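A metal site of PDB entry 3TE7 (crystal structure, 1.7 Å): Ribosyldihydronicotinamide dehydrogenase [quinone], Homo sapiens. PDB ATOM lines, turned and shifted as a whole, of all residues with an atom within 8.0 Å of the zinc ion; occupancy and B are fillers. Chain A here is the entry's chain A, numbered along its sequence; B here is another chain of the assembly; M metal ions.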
ATOM      1  N   TYR A 131      28.917  -6.044  13.846  1.00  0.00           N
ATOM      2  CA  TYR A 131      28.623  -6.858  15.032  1.00  0.00           C
ATOM      3  C   TYR A 131      29.319  -8.220  14.956  1.00  0.00           C
ATOM      4  O   TYR A 131      30.541  -8.257  14.823  1.00  0.00           O
ATOM      5  CB  TYR A 131      27.103  -6.942  15.301  1.00  0.00           C
ATOM      6  CG  TYR A 131      26.566  -5.623  15.822  1.00  0.00           C
ATOM      7  CD1 TYR A 131      27.108  -5.045  16.950  1.00  0.00           C
ATOM      8  CD2 TYR A 131      25.545  -4.949  15.169  1.00  0.00           C
ATOM      9  CE1 TYR A 131      26.655  -3.848  17.435  1.00  0.00           C
ATOM     10  CE2 TYR A 131      25.067  -3.732  15.656  1.00  0.00           C
ATOM     11  CZ  TYR A 131      25.640  -3.193  16.792  1.00  0.00           C
ATOM     12  OH  TYR A 131      25.199  -2.004  17.316  1.00  0.00           O
ATOM     13  N   ASP A 132      28.590  -9.331  15.030  1.00  0.00           N
ATOM     14  CA  ASP A 132      29.272 -10.626  15.025  1.00  0.00           C
ATOM     15  C   ASP A 132      30.089 -10.836  13.746  1.00  0.00           C
ATOM     16  O   ASP A 132      31.060 -11.590  13.744  1.00  0.00           O
ATOM     17  CB  ASP A 132      28.289 -11.779  15.250  1.00  0.00           C
ATOM     18  CG  ASP A 132      27.731 -11.801  16.666  1.00  0.00           C
ATOM     19  OD1 ASP A 132      28.273 -11.105  17.542  1.00  0.00           O
ATOM     20  OD2 ASP A 132      26.742 -12.531  16.893  1.00  0.00           O
ATOM     21  N   TRP A 168      27.680   0.871  27.381  1.00  0.00           N
ATOM     22  CA  TRP A 168      26.975   0.468  26.164  1.00  0.00           C
ATOM     23  C   TRP A 168      27.550   1.042  24.852  1.00  0.00           C
ATOM     24  O   TRP A 168      27.825   0.290  23.933  1.00  0.00           O
ATOM     25  CB  TRP A 168      25.481   0.794  26.305  1.00  0.00           C
ATOM     26  CG  TRP A 168      24.615   0.564  25.107  1.00  0.00           C
ATOM     27  CD1 TRP A 168      24.038   1.527  24.321  1.00  0.00           C
ATOM     28  CD2 TRP A 168      24.157  -0.691  24.595  1.00  0.00           C
ATOM     29  NE1 TRP A 168      23.271   0.940  23.331  1.00  0.00           N
ATOM     30  CE2 TRP A 168      23.325  -0.423  23.486  1.00  0.00           C
ATOM     31  CE3 TRP A 168      24.376  -2.022  24.967  1.00  0.00           C
ATOM     32  CZ2 TRP A 168      22.716  -1.432  22.739  1.00  0.00           C
ATOM     33  CZ3 TRP A 168      23.773  -3.028  24.213  1.00  0.00           C
ATOM     34  CH2 TRP A 168      22.947  -2.724  23.131  1.00  0.00           C
ATOM     35  N   LEU A 170      30.500   2.068  24.234  1.00  0.00           N
ATOM     36  CA  LEU A 170      31.873   1.619  24.020  1.00  0.00           C
ATOM     37  C   LEU A 170      31.933   0.120  23.727  1.00  0.00           C
ATOM     38  O   LEU A 170      32.509  -0.306  22.722  1.00  0.00           O
ATOM     39  CB  LEU A 170      32.745   1.950  25.254  1.00  0.00           C
ATOM     40  CG  LEU A 170      32.718   3.426  25.689  1.00  0.00           C
ATOM     41  CD1 LEU A 170      33.396   3.577  27.051  1.00  0.00           C
ATOM     42  CD2 LEU A 170      33.414   4.281  24.654  1.00  0.00           C
ATOM     43  N   GLN A 171      31.344  -0.679  24.609  1.00  0.00           N
ATOM     44  CA  GLN A 171      31.387  -2.139  24.448  1.00  0.00           C
ATOM     45  C   GLN A 171      30.547  -2.628  23.274  1.00  0.00           C
ATOM     46  O   GLN A 171      31.015  -3.437  22.467  1.00  0.00           O
ATOM     47  CB  GLN A 171      30.964  -2.841  25.743  1.00  0.00           C
ATOM     48  CG  GLN A 171      31.956  -2.625  26.889  1.00  0.00           C
ATOM     49  CD  GLN A 171      31.660  -3.479  28.143  1.00  0.00           C
ATOM     50  OE1 GLN A 171      32.572  -3.763  28.921  1.00  0.00           O
ATOM     51  NE2 GLN A 171      30.398  -3.880  28.325  1.00  0.00           N
ATOM     52  N   HIS A 172      29.328  -2.119  23.171  1.00  0.00           N
ATOM     53  CA  HIS A 172      28.433  -2.576  22.115  1.00  0.00           C
ATOM     54  C   HIS A 172      28.548  -1.756  20.828  1.00  0.00           C
ATOM     55  O   HIS A 172      28.787  -2.310  19.745  1.00  0.00           O
ATOM     56  CB  HIS A 172      26.984  -2.566  22.574  1.00  0.00           C
ATOM     57  CG  HIS A 172      26.039  -3.145  21.563  1.00  0.00           C
ATOM     58  ND1 HIS A 172      26.032  -4.494  21.249  1.00  0.00           N
ATOM     59  CD2 HIS A 172      25.130  -2.569  20.748  1.00  0.00           C
ATOM     60  CE1 HIS A 172      25.121  -4.719  20.316  1.00  0.00           C
ATOM     61  NE2 HIS A 172      24.568  -3.568  19.993  1.00  0.00           N
ATOM     62  N   GLY A 173      28.374  -0.446  20.953  1.00  0.00           N
ATOM     63  CA  GLY A 173      28.305   0.419  19.786  1.00  0.00           C
ATOM     64  C   GLY A 173      29.612   0.482  19.026  1.00  0.00           C
ATOM     65  O   GLY A 173      29.622   0.716  17.819  1.00  0.00           O
ATOM     66  N   THR A 174      30.720   0.290  19.734  1.00  0.00           N
ATOM     67  CA  THR A 174      32.045   0.394  19.111  1.00  0.00           C
ATOM     68  C   THR A 174      32.731  -0.973  18.990  1.00  0.00           C
ATOM     69  O   THR A 174      32.911  -1.499  17.896  1.00  0.00           O
ATOM     70  CB  THR A 174      32.945   1.364  19.927  1.00  0.00           C
ATOM     71  OG1 THR A 174      32.246   2.588  20.164  1.00  0.00           O
ATOM     72  CG2 THR A 174      34.244   1.670  19.184  1.00  0.00           C
ATOM     73  N   LEU A 175      33.107  -1.560  20.126  1.00  0.00           N
ATOM     74  CA  LEU A 175      33.889  -2.795  20.089  1.00  0.00           C
ATOM     75  C   LEU A 175      33.140  -3.971  19.454  1.00  0.00           C
ATOM     76  O   LEU A 175      33.648  -4.592  18.525  1.00  0.00           O
ATOM     77  CB  LEU A 175      34.392  -3.140  21.483  1.00  0.00           C
ATOM     78  CG  LEU A 175      35.301  -2.042  22.062  1.00  0.00           C
ATOM     79  CD1 LEU A 175      35.596  -2.331  23.528  1.00  0.00           C
ATOM     80  CD2 LEU A 175      36.588  -1.904  21.236  1.00  0.00           C
ATOM     81  N   HIS A 176      31.943  -4.285  19.941  1.00  0.00           N
ATOM     82  CA  HIS A 176      31.162  -5.396  19.376  1.00  0.00           C
ATOM     83  C   HIS A 176      30.844  -5.100  17.906  1.00  0.00           C
ATOM     84  O   HIS A 176      30.888  -6.005  17.078  1.00  0.00           O
ATOM     85  CB  HIS A 176      29.864  -5.598  20.183  1.00  0.00           C
ATOM     86  CG  HIS A 176      29.094  -6.820  19.793  1.00  0.00           C
ATOM     87  ND1 HIS A 176      27.936  -7.187  20.440  1.00  0.00           N
ATOM     88  CD2 HIS A 176      29.294  -7.744  18.832  1.00  0.00           C
ATOM     89  CE1 HIS A 176      27.451  -8.292  19.884  1.00  0.00           C
ATOM     90  NE2 HIS A 176      28.257  -8.646  18.908  1.00  0.00           N
ATOM     91  N   PHE A 177      30.533  -3.843  17.597  1.00  0.00           N
ATOM     92  CA  PHE A 177      30.238  -3.461  16.203  1.00  0.00           C
ATOM     93  C   PHE A 177      31.365  -3.852  15.250  1.00  0.00           C
ATOM     94  O   PHE A 177      31.123  -4.306  14.129  1.00  0.00           O
ATOM     95  CB  PHE A 177      29.923  -1.963  16.083  1.00  0.00           C
ATOM     96  CG  PHE A 177      29.410  -1.553  14.732  1.00  0.00           C
ATOM     97  CD1 PHE A 177      28.059  -1.668  14.427  1.00  0.00           C
ATOM     98  CD2 PHE A 177      30.266  -1.049  13.770  1.00  0.00           C
ATOM     99  CE1 PHE A 177      27.574  -1.305  13.185  1.00  0.00           C
ATOM    100  CE2 PHE A 177      29.793  -0.678  12.514  1.00  0.00           C
ATOM    101  CZ  PHE A 177      28.437  -0.810  12.210  1.00  0.00           C
ATOM    102  N   PHE A 180      34.841  -7.403  17.825  1.00  0.00           N
ATOM    103  CA  PHE A 180      35.570  -7.844  19.003  1.00  0.00           C
ATOM    104  C   PHE A 180      34.649  -8.675  19.887  1.00  0.00           C
ATOM    105  O   PHE A 180      33.438  -8.428  19.927  1.00  0.00           O
ATOM    106  CB  PHE A 180      36.024  -6.659  19.886  1.00  0.00           C
ATOM    107  CG  PHE A 180      37.238  -5.906  19.389  1.00  0.00           C
ATOM    108  CD1 PHE A 180      37.100  -4.698  18.731  1.00  0.00           C
ATOM    109  CD2 PHE A 180      38.524  -6.381  19.658  1.00  0.00           C
ATOM    110  CE1 PHE A 180      38.229  -3.984  18.311  1.00  0.00           C
ATOM    111  CE2 PHE A 180      39.641  -5.675  19.251  1.00  0.00           C
ATOM    112  CZ  PHE A 180      39.506  -4.480  18.572  1.00  0.00           C
ATOM    113  N   VAL A 182      34.098  -9.102  23.860  1.00  0.00           N
ATOM    114  CA  VAL A 182      34.391  -8.166  24.923  1.00  0.00           C
ATOM    115  C   VAL A 182      34.564  -8.917  26.248  1.00  0.00           C
ATOM    116  O   VAL A 182      33.669  -9.619  26.696  1.00  0.00           O
ATOM    117  CB  VAL A 182      33.271  -7.108  25.037  1.00  0.00           C
ATOM    118  CG1 VAL A 182      33.531  -6.152  26.202  1.00  0.00           C
ATOM    119  CG2 VAL A 182      33.137  -6.349  23.725  1.00  0.00           C
ATOM    120  N   ILE A 219      31.880 -11.581  27.656  1.00  0.00           N
ATOM    121  CA  ILE A 219      30.511 -11.389  28.121  1.00  0.00           C
ATOM    122  C   ILE A 219      29.571 -11.518  26.940  1.00  0.00           C
ATOM    123  O   ILE A 219      29.986 -11.429  25.791  1.00  0.00           O
ATOM    124  CB  ILE A 219      30.305  -9.989  28.700  1.00  0.00           C
ATOM    125  CG1 ILE A 219      30.532  -8.924  27.613  1.00  0.00           C
ATOM    126  CG2 ILE A 219      31.227  -9.758  29.877  1.00  0.00           C
ATOM    127  CD1 ILE A 219      30.155  -7.534  28.044  1.00  0.00           C
ATOM    128  N   PRO A 220      28.287 -11.760  27.228  1.00  0.00           N
ATOM    129  CA  PRO A 220      27.255 -11.635  26.200  1.00  0.00           C
ATOM    130  C   PRO A 220      26.991 -10.148  26.017  1.00  0.00           C
ATOM    131  O   PRO A 220      26.328  -9.516  26.843  1.00  0.00           O
ATOM    132  CB  PRO A 220      26.046 -12.332  26.829  1.00  0.00           C
ATOM    133  CG  PRO A 220      26.265 -12.202  28.302  1.00  0.00           C
ATOM    134  CD  PRO A 220      27.748 -12.218  28.523  1.00  0.00           C
ATOM    135  N   CYS A 221      27.553  -9.574  24.955  1.00  0.00           N
ATOM    136  CA  CYS A 221      27.458  -8.135  24.758  1.00  0.00           C
ATOM    137  C   CYS A 221      26.092  -7.775  24.171  1.00  0.00           C
ATOM    138  O   CYS A 221      25.958  -7.511  22.975  1.00  0.00           O
ATOM    139  CB  CYS A 221      28.595  -7.625  23.867  1.00  0.00           C
ATOM    140  SG  CYS A 221      28.655  -5.818  23.803  1.00  0.00           S
ATOM    141  N   THR A 222      25.082  -7.775  25.035  1.00  0.00           N
ATOM    142  CA  THR A 222      23.702  -7.573  24.615  1.00  0.00           C
ATOM    143  C   THR A 222      23.004  -6.481  25.422  1.00  0.00           C
ATOM    144  O   THR A 222      23.507  -6.069  26.457  1.00  0.00           O
ATOM    145  CB  THR A 222      22.907  -8.872  24.786  1.00  0.00           C
ATOM    146  OG1 THR A 222      22.816  -9.185  26.188  1.00  0.00           O
ATOM    147  CG2 THR A 222      23.591 -10.011  24.060  1.00  0.00           C
ATOM    148  N   ALA A 223      21.837  -6.030  24.951  1.00  0.00           N
ATOM    149  CA  ALA A 223      21.039  -5.091  25.718  1.00  0.00           C
ATOM    150  C   ALA A 223      20.730  -5.672  27.093  1.00  0.00           C
ATOM    151  O   ALA A 223      20.790  -4.971  28.103  1.00  0.00           O
ATOM    152  CB  ALA A 223      19.730  -4.751  24.990  1.00  0.00           C
ATOM    153  N   TRP A 225      22.421  -7.797  28.963  1.00  0.00           N
ATOM    154  CA  TRP A 225      23.579  -7.745  29.853  1.00  0.00           C
ATOM    155  C   TRP A 225      23.734  -6.324  30.392  1.00  0.00           C
ATOM    156  O   TRP A 225      23.994  -6.113  31.585  1.00  0.00           O
ATOM    157  CB  TRP A 225      24.847  -8.199  29.127  1.00  0.00           C
ATOM    158  CG  TRP A 225      26.038  -8.313  30.028  1.00  0.00           C
ATOM    159  CD1 TRP A 225      26.453  -9.413  30.707  1.00  0.00           C
ATOM    160  CD2 TRP A 225      26.978  -7.268  30.343  1.00  0.00           C
ATOM    161  NE1 TRP A 225      27.599  -9.136  31.413  1.00  0.00           N
ATOM    162  CE2 TRP A 225      27.934  -7.820  31.220  1.00  0.00           C
ATOM    163  CE3 TRP A 225      27.096  -5.926  29.979  1.00  0.00           C
ATOM    164  CZ2 TRP A 225      29.002  -7.089  31.722  1.00  0.00           C
ATOM    165  CZ3 TRP A 225      28.154  -5.192  30.472  1.00  0.00           C
ATOM    166  CH2 TRP A 225      29.095  -5.769  31.348  1.00  0.00           C
ATOM    167  N   HIS A 226      23.566  -5.337  29.523  1.00  0.00           N
ATOM    168  CA  HIS A 226      23.774  -3.953  29.923  1.00  0.00           C
ATOM    169  C   HIS A 226      22.649  -3.362  30.767  1.00  0.00           C
ATOM    170  O   HIS A 226      22.913  -2.590  31.703  1.00  0.00           O
ATOM    171  CB  HIS A 226      24.040  -3.066  28.690  1.00  0.00           C
ATOM    172  CG  HIS A 226      25.380  -3.284  28.073  1.00  0.00           C
ATOM    173  ND1 HIS A 226      25.642  -4.302  27.179  1.00  0.00           N
ATOM    174  CD2 HIS A 226      26.542  -2.604  28.205  1.00  0.00           C
ATOM    175  CE1 HIS A 226      26.905  -4.238  26.793  1.00  0.00           C
ATOM    176  NE2 HIS A 226      27.464  -3.207  27.395  1.00  0.00           N
ATOM    177  N   VAL B 159      19.120  -4.101  16.368  1.00  0.00           N
ATOM    178  CA  VAL B 159      20.551  -4.380  16.515  1.00  0.00           C
ATOM    179  C   VAL B 159      21.304  -3.331  17.338  1.00  0.00           C
ATOM    180  O   VAL B 159      22.230  -3.651  18.078  1.00  0.00           O
ATOM    181  CB  VAL B 159      21.269  -4.571  15.147  1.00  0.00           C
ATOM    182  CG1 VAL B 159      20.884  -5.904  14.537  1.00  0.00           C
ATOM    183  CG2 VAL B 159      20.952  -3.416  14.214  1.00  0.00           C
HETATM  184 ZN    ZN M   1      27.239  -6.009  22.073  1.00  0.00          ZN
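The side-chain hydroxyl (OH) of Tyr 131 sits at hydrogen-bond distance from a ring nitrogen (NE2) of His 172 (3.2 Å). O of His 172 is in hydrogen-bond range of N of Phe 177 (3.2 Å). The backbone carbonyl oxygen (O) of Val 159 of chain B is in hydrogen-bond range of a ring nitrogen (NE2) of His 172. The backbone NH (N) of His 176 sits at hydrogen-bond distance from the backbone carbonyl oxygen (O) of Gln 171. NE2 of His 176 is in hydrogen-bond range of OD1 of Asp 132 (2.8 Å). SG of Cys 221 lies close to O of Gln 171, 3.6 Å away.
Three residues have an atom within 4 Å of the zinc ion: His 172, His 176 and Cys 221. The nearest printed residue that does not touch the zinc ion is Thr 222 (4.1 Å).
The zinc ion is bound by ND1 of His 172, ND1 of His 176, O of Cys 221 and SG of Cys 221.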
